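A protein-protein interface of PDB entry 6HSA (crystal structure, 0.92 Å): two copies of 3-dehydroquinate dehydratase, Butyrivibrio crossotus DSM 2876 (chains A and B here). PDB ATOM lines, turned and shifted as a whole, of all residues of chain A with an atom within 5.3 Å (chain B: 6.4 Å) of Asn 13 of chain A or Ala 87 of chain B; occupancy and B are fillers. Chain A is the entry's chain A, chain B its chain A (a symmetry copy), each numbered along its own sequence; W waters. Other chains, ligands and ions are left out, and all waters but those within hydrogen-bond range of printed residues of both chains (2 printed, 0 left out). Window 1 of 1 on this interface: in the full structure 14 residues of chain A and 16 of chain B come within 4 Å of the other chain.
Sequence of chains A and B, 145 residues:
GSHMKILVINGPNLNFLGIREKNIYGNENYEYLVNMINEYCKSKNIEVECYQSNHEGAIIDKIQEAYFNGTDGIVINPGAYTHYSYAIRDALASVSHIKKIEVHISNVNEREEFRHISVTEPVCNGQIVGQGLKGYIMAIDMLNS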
ATOM      1  N   GLY A  11     -17.869   6.278 -13.552  1.00  0.00           N
ATOM      2  CA  GLY A  11     -17.872   5.377 -14.675  1.00  0.00           C
ATOM      3  C   GLY A  11     -16.844   4.270 -14.571  1.00  0.00           C
ATOM      4  O   GLY A  11     -16.426   3.863 -13.474  1.00  0.00           O
ATOM      5  N   PRO A  12     -16.457   3.695 -15.721  1.00  0.00           N
ATOM      6  CA  PRO A  12     -15.714   2.450 -15.706  1.00  0.00           C
ATOM      7  C   PRO A  12     -14.377   2.644 -15.003  1.00  0.00           C
ATOM      8  O   PRO A  12     -13.719   3.676 -15.114  1.00  0.00           O
ATOM      9  CB  PRO A  12     -15.532   2.108 -17.195  1.00  0.00           C
ATOM     10  CG  PRO A  12     -15.700   3.436 -17.895  1.00  0.00           C
ATOM     11  CD  PRO A  12     -16.808   4.110 -17.082  1.00  0.00           C
ATOM     12  N   ASN A  13     -13.971   1.567 -14.313  1.00  0.00           N
ATOM     13  CA  ASN A  13     -12.668   1.432 -13.680  1.00  0.00           C
ATOM     14  C   ASN A  13     -12.510   2.253 -12.397  1.00  0.00           C
ATOM     15  O   ASN A  13     -11.539   2.056 -11.669  1.00  0.00           O
ATOM     16  CB  ASN A  13     -11.521   1.740 -14.641  1.00  0.00           C
ATOM     17  CG  ASN A  13     -11.622   0.867 -15.882  1.00  0.00           C
ATOM     18  OD1 ASN A  13     -11.571  -0.353 -15.801  1.00  0.00           O
ATOM     19  ND2 ASN A  13     -11.830   1.493 -17.043  1.00  0.00           N
ATOM     20  N   LEU A  14     -13.475   3.135 -12.055  1.00  0.00           N
ATOM     21  CA  LEU A  14     -13.303   3.982 -10.880  1.00  0.00           C
ATOM     22  C   LEU A  14     -13.514   3.215  -9.577  1.00  0.00           C
ATOM     23  O   LEU A  14     -13.049   3.645  -8.529  1.00  0.00           O
ATOM     24  CB  LEU A  14     -14.188   5.222 -11.015  1.00  0.00           C
ATOM     25  CG  LEU A  14     -13.508   6.257 -11.950  1.00  0.00           C
ATOM     26  CD1 LEU A  14     -14.513   7.046 -12.759  1.00  0.00           C
ATOM     27  CD2 LEU A  14     -12.561   7.125 -11.163  1.00  0.00           C
ATOM     28  N   ASN A  15     -14.209   2.065  -9.653  1.00  0.00           N
ATOM     29  CA  ASN A  15     -14.244   1.172  -8.494  1.00  0.00           C
ATOM     30  C   ASN A  15     -12.874   0.556  -8.165  1.00  0.00           C
ATOM     31  O   ASN A  15     -12.753  -0.046  -7.103  1.00  0.00           O
ATOM     32  CB  ASN A  15     -15.300   0.074  -8.691  1.00  0.00           C
ATOM     33  CG  ASN A  15     -15.047  -0.770  -9.925  1.00  0.00           C
ATOM     34  OD1 ASN A  15     -14.675  -0.270 -10.979  1.00  0.00           O
ATOM     35  ND2 ASN A  15     -15.306  -2.069  -9.802  1.00  0.00           N
ATOM     36  N   PHE A  16     -11.884   0.699  -9.046  1.00  0.00           N
ATOM     37  CA  PHE A  16     -10.532   0.216  -8.815  1.00  0.00           C
ATOM     38  C   PHE A  16      -9.586   1.330  -8.358  1.00  0.00           C
ATOM     39  O   PHE A  16      -8.375   1.138  -8.366  1.00  0.00           O
ATOM     40  CB  PHE A  16      -9.979  -0.551 -10.032  1.00  0.00           C
ATOM     41  CG  PHE A  16     -10.206  -2.042  -9.984  1.00  0.00           C
ATOM     42  CD1 PHE A  16     -11.326  -2.619  -9.417  1.00  0.00           C
ATOM     43  CD2 PHE A  16      -9.247  -2.890 -10.524  1.00  0.00           C
ATOM     44  CE1 PHE A  16     -11.483  -3.978  -9.375  1.00  0.00           C
ATOM     45  CE2 PHE A  16      -9.406  -4.281 -10.483  1.00  0.00           C
ATOM     46  CZ  PHE A  16     -10.513  -4.816  -9.887  1.00  0.00           C
ATOM     47  N   LEU A  17     -10.102   2.450  -7.858  1.00  0.00           N
ATOM     48  CA  LEU A  17      -9.246   3.372  -7.123  1.00  0.00           C
ATOM     49  C   LEU A  17      -8.467   2.627  -6.041  1.00  0.00           C
ATOM     50  O   LEU A  17      -8.976   1.708  -5.424  1.00  0.00           O
ATOM     51  CB  LEU A  17     -10.084   4.501  -6.508  1.00  0.00           C
ATOM     52  CG  LEU A  17     -10.570   5.535  -7.511  1.00  0.00           C
ATOM     53  CD1 LEU A  17     -11.605   6.416  -6.853  1.00  0.00           C
ATOM     54  CD2 LEU A  17      -9.451   6.313  -8.114  1.00  0.00           C
ATOM     55  N   ARG A  20      -5.467   0.890  -8.841  1.00  0.00           N
ATOM     56  CA  ARG A  20      -4.794   1.720  -9.854  1.00  0.00           C
ATOM     57  C   ARG A  20      -3.684   2.618  -9.318  1.00  0.00           C
ATOM     58  O   ARG A  20      -3.455   2.749  -8.134  1.00  0.00           O
ATOM     59  CB  ARG A  20      -5.842   2.503 -10.626  1.00  0.00           C
ATOM     60  CG  ARG A  20      -6.764   1.567 -11.343  1.00  0.00           C
ATOM     61  CD  ARG A  20      -8.087   2.313 -11.854  1.00  0.00           C
ATOM     62  NE  ARG A  20      -7.844   3.222 -12.951  1.00  0.00           N
ATOM     63  CZ  ARG A  20      -8.692   4.121 -13.470  1.00  0.00           C
ATOM     64  NH1 ARG A  20      -9.826   4.301 -12.864  1.00  0.00           N
ATOM     65  NH2 ARG A  20      -8.398   4.788 -14.552  1.00  0.00           N
ATOM     66  N   GLN A  52     -21.731   3.557  -9.202  1.00  0.00           N
ATOM     67  CA  GLN A  52     -20.624   3.278 -10.126  1.00  0.00           C
ATOM     68  C   GLN A  52     -21.041   2.137 -11.031  1.00  0.00           C
ATOM     69  O   GLN A  52     -21.687   1.176 -10.591  1.00  0.00           O
ATOM     70  CB  GLN A  52     -19.358   2.936  -9.337  1.00  0.00           C
ATOM     71  CG  GLN A  52     -18.091   2.796 -10.213  1.00  0.00           C
ATOM     72  CD  GLN A  52     -17.906   1.449 -10.879  1.00  0.00           C
ATOM     73  OE1 GLN A  52     -18.293   0.407 -10.351  1.00  0.00           O
ATOM     74  NE2 GLN A  52     -17.259   1.460 -12.034  1.00  0.00           N
ATOM     75  N   ASN A  54     -19.350   0.000 -14.802  1.00  0.00           N
ATOM     76  CA  ASN A  54     -18.484  -0.092 -15.958  1.00  0.00           C
ATOM     77  C   ASN A  54     -19.254  -0.059 -17.280  1.00  0.00           C
ATOM     78  O   ASN A  54     -18.615  -0.019 -18.339  1.00  0.00           O
ATOM     79  CB  ASN A  54     -17.634  -1.352 -15.896  1.00  0.00           C
ATOM     80  CG  ASN A  54     -16.755  -1.381 -14.657  1.00  0.00           C
ATOM     81  OD1 ASN A  54     -16.174  -0.357 -14.277  1.00  0.00           O
ATOM     82  ND2 ASN A  54     -16.642  -2.542 -14.049  1.00  0.00           N
ATOM     83  N   ALA A  80     -13.053   6.559 -18.843  1.00  0.00           N
ATOM     84  CA  ALA A  80     -12.568   6.710 -20.213  1.00  0.00           C
ATOM     85  C   ALA A  80     -13.682   7.054 -21.189  1.00  0.00           C
ATOM     86  O   ALA A  80     -13.406   7.584 -22.272  1.00  0.00           O
ATOM     87  CB  ALA A  80     -11.870   5.443 -20.653  1.00  0.00           C
ATOM     88  N   TYR A  81     -14.950   6.744 -20.852  1.00  0.00           N
ATOM     89  CA  TYR A  81     -16.074   7.132 -21.703  1.00  0.00           C
ATOM     90  C   TYR A  81     -16.135   8.624 -21.969  1.00  0.00           C
ATOM     91  O   TYR A  81     -16.743   9.064 -22.948  1.00  0.00           O
ATOM     92  CB  TYR A  81     -17.404   6.683 -21.097  1.00  0.00           C
ATOM     93  CG  TYR A  81     -17.627   5.180 -21.050  1.00  0.00           C
ATOM     94  CD1 TYR A  81     -17.182   4.320 -22.035  1.00  0.00           C
ATOM     95  CD2 TYR A  81     -18.338   4.619 -19.995  1.00  0.00           C
ATOM     96  CE1 TYR A  81     -17.372   2.951 -21.948  1.00  0.00           C
ATOM     97  CE2 TYR A  81     -18.563   3.247 -19.911  1.00  0.00           C
ATOM     98  CZ  TYR A  81     -18.050   2.410 -20.886  1.00  0.00           C
ATOM     99  OH  TYR A  81     -18.164   1.054 -20.836  1.00  0.00           O
ATOM    100  N   TYR A  84     -15.184   9.486 -25.641  1.00  0.00           N
ATOM    101  CA  TYR A  84     -15.812   8.919 -26.827  1.00  0.00           C
ATOM    102  C   TYR A  84     -17.303   8.682 -26.712  1.00  0.00           C
ATOM    103  O   TYR A  84     -17.939   8.445 -27.745  1.00  0.00           O
ATOM    104  CB  TYR A  84     -15.091   7.642 -27.313  1.00  0.00           C
ATOM    105  CG  TYR A  84     -15.079   6.467 -26.363  1.00  0.00           C
ATOM    106  CD1 TYR A  84     -14.160   6.396 -25.317  1.00  0.00           C
ATOM    107  CD2 TYR A  84     -15.898   5.357 -26.552  1.00  0.00           C
ATOM    108  CE1 TYR A  84     -14.069   5.267 -24.508  1.00  0.00           C
ATOM    109  CE2 TYR A  84     -15.813   4.229 -25.772  1.00  0.00           C
ATOM    110  CZ  TYR A  84     -14.861   4.163 -24.754  1.00  0.00           C
ATOM    111  OH  TYR A  84     -14.649   3.058 -23.992  1.00  0.00           O
ATOM    112  N   GLU B  56     -19.437  -4.104 -23.616  1.00  0.00           N
ATOM    113  CA  GLU B  56     -18.179  -3.503 -23.200  1.00  0.00           C
ATOM    114  C   GLU B  56     -18.048  -3.554 -21.672  1.00  0.00           C
ATOM    115  O   GLU B  56     -16.986  -3.878 -21.128  1.00  0.00           O
ATOM    116  CB  GLU B  56     -18.160  -2.072 -23.734  1.00  0.00           C
ATOM    117  CG  GLU B  56     -16.920  -1.296 -23.491  1.00  0.00           C
ATOM    118  CD  GLU B  56     -16.949   0.108 -24.125  1.00  0.00           C
ATOM    119  OE1 GLU B  56     -18.006   0.555 -24.543  1.00  0.00           O
ATOM    120  OE2 GLU B  56     -15.883   0.741 -24.219  1.00  0.00           O
ATOM    121  N   ILE B  60     -15.241  -5.425 -19.097  1.00  0.00           N
ATOM    122  CA  ILE B  60     -14.521  -4.747 -18.030  1.00  0.00           C
ATOM    123  C   ILE B  60     -14.777  -5.440 -16.689  1.00  0.00           C
ATOM    124  O   ILE B  60     -13.825  -5.674 -15.924  1.00  0.00           O
ATOM    125  CB  ILE B  60     -14.921  -3.254 -17.982  1.00  0.00           C
ATOM    126  CG1 ILE B  60     -14.480  -2.561 -19.276  1.00  0.00           C
ATOM    127  CG2 ILE B  60     -14.313  -2.580 -16.756  1.00  0.00           C
ATOM    128  CD1 ILE B  60     -15.079  -1.177 -19.480  1.00  0.00           C
ATOM    129  N   GLN B  64     -11.906  -7.138 -14.237  1.00  0.00           N
ATOM    130  CA  GLN B  64     -11.788  -6.815 -12.805  1.00  0.00           C
ATOM    131  C   GLN B  64     -11.918  -8.068 -11.932  1.00  0.00           C
ATOM    132  O   GLN B  64     -11.194  -8.225 -10.960  1.00  0.00           O
ATOM    133  CB  GLN B  64     -12.847  -5.793 -12.416  1.00  0.00           C
ATOM    134  CG  GLN B  64     -12.571  -4.429 -13.033  1.00  0.00           C
ATOM    135  CD  GLN B  64     -13.526  -3.371 -12.534  1.00  0.00           C
ATOM    136  OE1 GLN B  64     -14.684  -3.679 -12.163  1.00  0.00           O
ATOM    137  NE2 GLN B  64     -13.080  -2.134 -12.498  1.00  0.00           N
ATOM    138  N   TYR B  84     -11.675   1.412 -30.324  1.00  0.00           N
ATOM    139  CA  TYR B  84     -12.239   2.600 -29.700  1.00  0.00           C
ATOM    140  C   TYR B  84     -12.436   2.506 -28.201  1.00  0.00           C
ATOM    141  O   TYR B  84     -12.667   3.545 -27.574  1.00  0.00           O
ATOM    142  CB  TYR B  84     -13.541   3.061 -30.393  1.00  0.00           C
ATOM    143  CG  TYR B  84     -14.705   2.098 -30.359  1.00  0.00           C
ATOM    144  CD1 TYR B  84     -14.788   1.036 -31.260  1.00  0.00           C
ATOM    145  CD2 TYR B  84     -15.795   2.286 -29.513  1.00  0.00           C
ATOM    146  CE1 TYR B  84     -15.909   0.213 -31.309  1.00  0.00           C
ATOM    147  CE2 TYR B  84     -16.915   1.492 -29.556  1.00  0.00           C
ATOM    148  CZ  TYR B  84     -16.993   0.459 -30.490  1.00  0.00           C
ATOM    149  OH  TYR B  84     -18.095  -0.319 -30.661  1.00  0.00           O
ATOM    150  N   SER B  85     -12.392   1.310 -27.588  1.00  0.00           N
ATOM    151  CA  SER B  85     -12.711   1.198 -26.164  1.00  0.00           C
ATOM    152  C   SER B  85     -11.520   1.539 -25.284  1.00  0.00           C
ATOM    153  O   SER B  85     -10.785   0.672 -24.786  1.00  0.00           O
ATOM    154  CB  SER B  85     -13.199  -0.189 -25.816  1.00  0.00           C
ATOM    155  OG  SER B  85     -13.503  -0.276 -24.431  1.00  0.00           O
ATOM    156  N   TYR B  86     -11.365   2.842 -25.014  1.00  0.00           N
ATOM    157  CA  TYR B  86     -10.411   3.252 -24.000  1.00  0.00           C
ATOM    158  C   TYR B  86     -10.810   2.743 -22.623  1.00  0.00           C
ATOM    159  O   TYR B  86      -9.965   2.616 -21.739  1.00  0.00           O
ATOM    160  CB  TYR B  86     -10.196   4.779 -24.021  1.00  0.00           C
ATOM    161  CG  TYR B  86      -9.465   5.241 -25.252  1.00  0.00           C
ATOM    162  CD1 TYR B  86      -8.086   5.048 -25.372  1.00  0.00           C
ATOM    163  CD2 TYR B  86     -10.104   5.852 -26.305  1.00  0.00           C
ATOM    164  CE1 TYR B  86      -7.390   5.464 -26.484  1.00  0.00           C
ATOM    165  CE2 TYR B  86      -9.404   6.269 -27.438  1.00  0.00           C
ATOM    166  CZ  TYR B  86      -8.047   6.092 -27.512  1.00  0.00           C
ATOM    167  OH  TYR B  86      -7.326   6.513 -28.597  1.00  0.00           O
ATOM    168  N   ALA B  87     -12.096   2.433 -22.405  1.00  0.00           N
ATOM    169  CA  ALA B  87     -12.512   1.869 -21.127  1.00  0.00           C
ATOM    170  C   ALA B  87     -11.957   0.449 -20.925  1.00  0.00           C
ATOM    171  O   ALA B  87     -11.509   0.128 -19.811  1.00  0.00           O
ATOM    172  CB  ALA B  87     -14.031   1.904 -20.991  1.00  0.00           C
ATOM    173  N   ILE B  88     -11.980  -0.395 -21.957  1.00  0.00           N
ATOM    174  CA  ILE B  88     -11.355  -1.713 -21.844  1.00  0.00           C
ATOM    175  C   ILE B  88      -9.847  -1.555 -21.712  1.00  0.00           C
ATOM    176  O   ILE B  88      -9.213  -2.286 -20.936  1.00  0.00           O
ATOM    177  CB  ILE B  88     -11.766  -2.635 -23.013  1.00  0.00           C
ATOM    178  CG1 ILE B  88     -13.233  -3.054 -22.856  1.00  0.00           C
ATOM    179  CG2 ILE B  88     -10.859  -3.864 -23.073  1.00  0.00           C
ATOM    180  CD1 ILE B  88     -13.820  -3.698 -24.094  1.00  0.00           C
ATOM    181  N   ARG B  89      -9.248  -0.613 -22.451  1.00  0.00           N
ATOM    182  CA  ARG B  89      -7.819  -0.361 -22.277  1.00  0.00           C
ATOM    183  C   ARG B  89      -7.491  -0.071 -20.805  1.00  0.00           C
ATOM    184  O   ARG B  89      -6.567  -0.656 -20.236  1.00  0.00           O
ATOM    185  CB  ARG B  89      -7.423   0.834 -23.162  1.00  0.00           C
ATOM    186  CG  ARG B  89      -5.959   1.226 -23.027  1.00  0.00           C
ATOM    187  CD  ARG B  89      -5.771   2.651 -23.428  1.00  0.00           C
ATOM    188  NE  ARG B  89      -4.396   3.107 -23.271  1.00  0.00           N
ATOM    189  CZ  ARG B  89      -3.584   3.441 -24.271  1.00  0.00           C
ATOM    190  NH1 ARG B  89      -3.931   3.213 -25.536  1.00  0.00           N
ATOM    191  NH2 ARG B  89      -2.429   4.019 -23.989  1.00  0.00           N
ATOM    192  N   ASP B  90      -8.232   0.868 -20.202  1.00  0.00           N
ATOM    193  CA  ASP B  90      -7.942   1.216 -18.820  1.00  0.00           C
ATOM    194  C   ASP B  90      -8.184   0.006 -17.886  1.00  0.00           C
ATOM    195  O   ASP B  90      -7.455  -0.127 -16.887  1.00  0.00           O
ATOM    196  CB  ASP B  90      -8.769   2.422 -18.384  1.00  0.00           C
ATOM    197  CG  ASP B  90      -8.238   3.766 -18.810  1.00  0.00           C
ATOM    198  OD1 ASP B  90      -7.078   3.838 -19.262  1.00  0.00           O
ATOM    199  OD2 ASP B  90      -8.998   4.750 -18.644  1.00  0.00           O
ATOM    200  N   ALA B  91      -9.166  -0.834 -18.179  1.00  0.00           N
ATOM    201  CA  ALA B  91      -9.371  -2.024 -17.366  1.00  0.00           C
ATOM    202  C   ALA B  91      -8.157  -2.941 -17.437  1.00  0.00           C
ATOM    203  O   ALA B  91      -7.671  -3.448 -16.415  1.00  0.00           O
ATOM    204  CB  ALA B  91     -10.621  -2.745 -17.822  1.00  0.00           C
ATOM    205  N   LEU B  92      -7.670  -3.193 -18.655  1.00  0.00           N
ATOM    206  CA  LEU B  92      -6.487  -4.050 -18.825  1.00  0.00           C
ATOM    207  C   LEU B  92      -5.284  -3.444 -18.086  1.00  0.00           C
ATOM    208  O   LEU B  92      -4.515  -4.160 -17.453  1.00  0.00           O
ATOM    209  CB  LEU B  92      -6.201  -4.202 -20.322  1.00  0.00           C
ATOM    210  CG  LEU B  92      -7.215  -5.038 -21.083  1.00  0.00           C
ATOM    211  CD1 LEU B  92      -7.016  -4.877 -22.581  1.00  0.00           C
ATOM    212  CD2 LEU B  92      -7.156  -6.522 -20.703  1.00  0.00           C
ATOM    213  N   SER B  94      -5.366  -1.609 -15.474  1.00  0.00           N
ATOM    214  CA  SER B  94      -5.616  -1.602 -14.039  1.00  0.00           C
ATOM    215  C   SER B  94      -5.178  -2.906 -13.350  1.00  0.00           C
ATOM    216  O   SER B  94      -5.016  -2.871 -12.153  1.00  0.00           O
ATOM    217  CB  SER B  94      -7.081  -1.320 -13.730  1.00  0.00           C
ATOM    218  OG  SER B  94      -7.933  -2.418 -13.925  1.00  0.00           O
HETATM  219  O   HOH W   1     -11.527   4.487 -17.449  1.00  0.00           O
HETATM  220  O   HOH W   2     -10.514  -1.339 -13.441  1.00  0.00           O
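The side-chain amide nitrogen (ND2) of Asn 13 of chain A is in hydrogen-bond range of the backbone carbonyl oxygen (O) of Ala 87 of chain B, at 3.1 Å. The side-chain amide oxygen (OD1) of Asn 13 of chain A sits close to the backbone NH (N) of Ala 91 of chain B (3.4 Å). The side-chain amide oxygen of Asn 15 of chain A lies within hydrogen-bond range of the side-chain amide nitrogen of Gln 64 of chain B (2.9 Å). The side-chain amide nitrogen (ND2) of Asn 54 of chain A is in hydrogen-bond range of the side-chain amide oxygen (OE1) of Gln 64 of chain B. The side-chain hydroxyl (OH) of Tyr 84 of chain A is in hydrogen-bond range of the side-chain carboxylate (OE2) of Glu 56 of chain B (2.6 Å). OH of Tyr 84 of chain A is in hydrogen-bond range of N of Tyr 86 of chain B, at 3.4 Å. The backbone NH (N) of Ala 87 of chain B sits at hydrogen-bond distance from the side-chain hydroxyl (OH) of Tyr 84 of chain A, at 3.1 Å.
The backbone carbonyl oxygen of Asn 13 of chain A is in hydrogen-bond range of the guanidinium group of Arg 20 of chain A, at 3.1 Å. OD1 of Asn 15 of chain A sits at hydrogen-bond distance from NE2 of Gln 52 of chain A (3.3 Å). The side-chain amide nitrogen (NE2) of Gln 52 of chain A sits at hydrogen-bond distance from the side-chain amide oxygen (OD1) of Asn 54 of chain A, 3.1 Å away. The backbone carbonyl oxygen (O) of Asn 54 of chain A is in hydrogen-bond range of the side-chain hydroxyl (OH) of Tyr 81 of chain A (2.8 Å). OG of Ser 85 of chain B is in hydrogen-bond range of OE2 of Glu 56 of chain B (2.6 Å). The side-chain hydroxyl (OG) of Ser 94 of chain B is in hydrogen-bond range of the backbone carbonyl oxygen (O) of Ala 91 of chain B (2.7 Å).
Among the printed residues, pairs that only touch across the chains: Asn 54 of chain A with Ile 60 of chain B, Tyr 84 of chain A with Ser 85 of chain B, Asn 13 of chain A with Asp 90 of chain B, Ala 80 of chain A with Ala 87 of chain B, Tyr 81 of chain A with Glu 56 of chain B, Ala 80 of chain A with Tyr 86 of chain B, Ala 80 of chain A with Asp 90 of chain B, Phe 16 of chain A with Gln 64 of chain B, Tyr 84 of chain A with Tyr 84 of chain B, Tyr 81 of chain A with Ala 87 of chain B, Asn 13 of chain A with Ile 60 of chain B, Phe 16 of chain A with Ser 94 of chain B, Arg 20 of chain A with Ser 94 of chain B, Asn 13 of chain A with Gln 64 of chain B and Pro 12 of chain A with Ala 87 of chain B.
Asn 13 of chain A touches just these residues of chain B: Ile 60 (3.7 Å), Gln 64 (3.8 Å), Ala 87 (3.1 Å), Asp 90 (3.5 Å) and Ala 91 (3.2 Å). Of chain A, only Pro 12 (3.8 Å), Asn 13 (3.1 Å), Ala 80 (3.5 Å), Tyr 81 (3.6 Å) and Tyr 84 (3.1 Å) come within 4 Å of Ala 87 of chain B. Of the printed residues of chain A, Ala 91 of chain B touches Asn 13 (3.2 Å). Printed residues of chain A within 4 Å of Ser 85 of chain B: Tyr 84. The nearest residue of chain B that does not touch Asn 13 of chain A is Ser 94 of chain B (4.6 Å). The nearest printed residue of chain A that does not touch Gln 64 of chain B is Leu 14 of chain A (5.3 Å).
Hydrophobic or aromatic side chains of chain B that line the printed part of chain A: Ile 60, Tyr 86, Ala 87 and Ala 91. Along chain B the printed residues that touch a printed residue of chain A span positions 56 to 94. Hydrophobic or aromatic side chains of chain A that line the printed part of chain B: Pro 12, Phe 16, Ala 80, Tyr 81 and Tyr 84. Among the printed residues, 22 pairs touch across the chains.
Tyr 84 of chain B touches its own counterpart, Tyr 84 of chain A. Of the 22 pairs that touch across the chains among the printed residues, 1 has its exchanged pair printed and touching as well.
Water W2 lies within hydrogen-bond range of the side-chain amide oxygen (OD1) of Asn 13 of chain A (2.8 Å), the side-chain hydroxyl (OG) of Ser 94 of chain B (2.8 Å) and the side-chain amide nitrogen (NE2) of Gln 64 of chain B (2.8 Å). Water W1 lies within hydrogen-bond range of the side-chain carboxylate of Asp 90 of chain B, the backbone NH of Ala 80 of chain A, the side-chain amide nitrogen of Asn 13 of chain A and the backbone carbonyl oxygen of Pro 12 of chain A.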
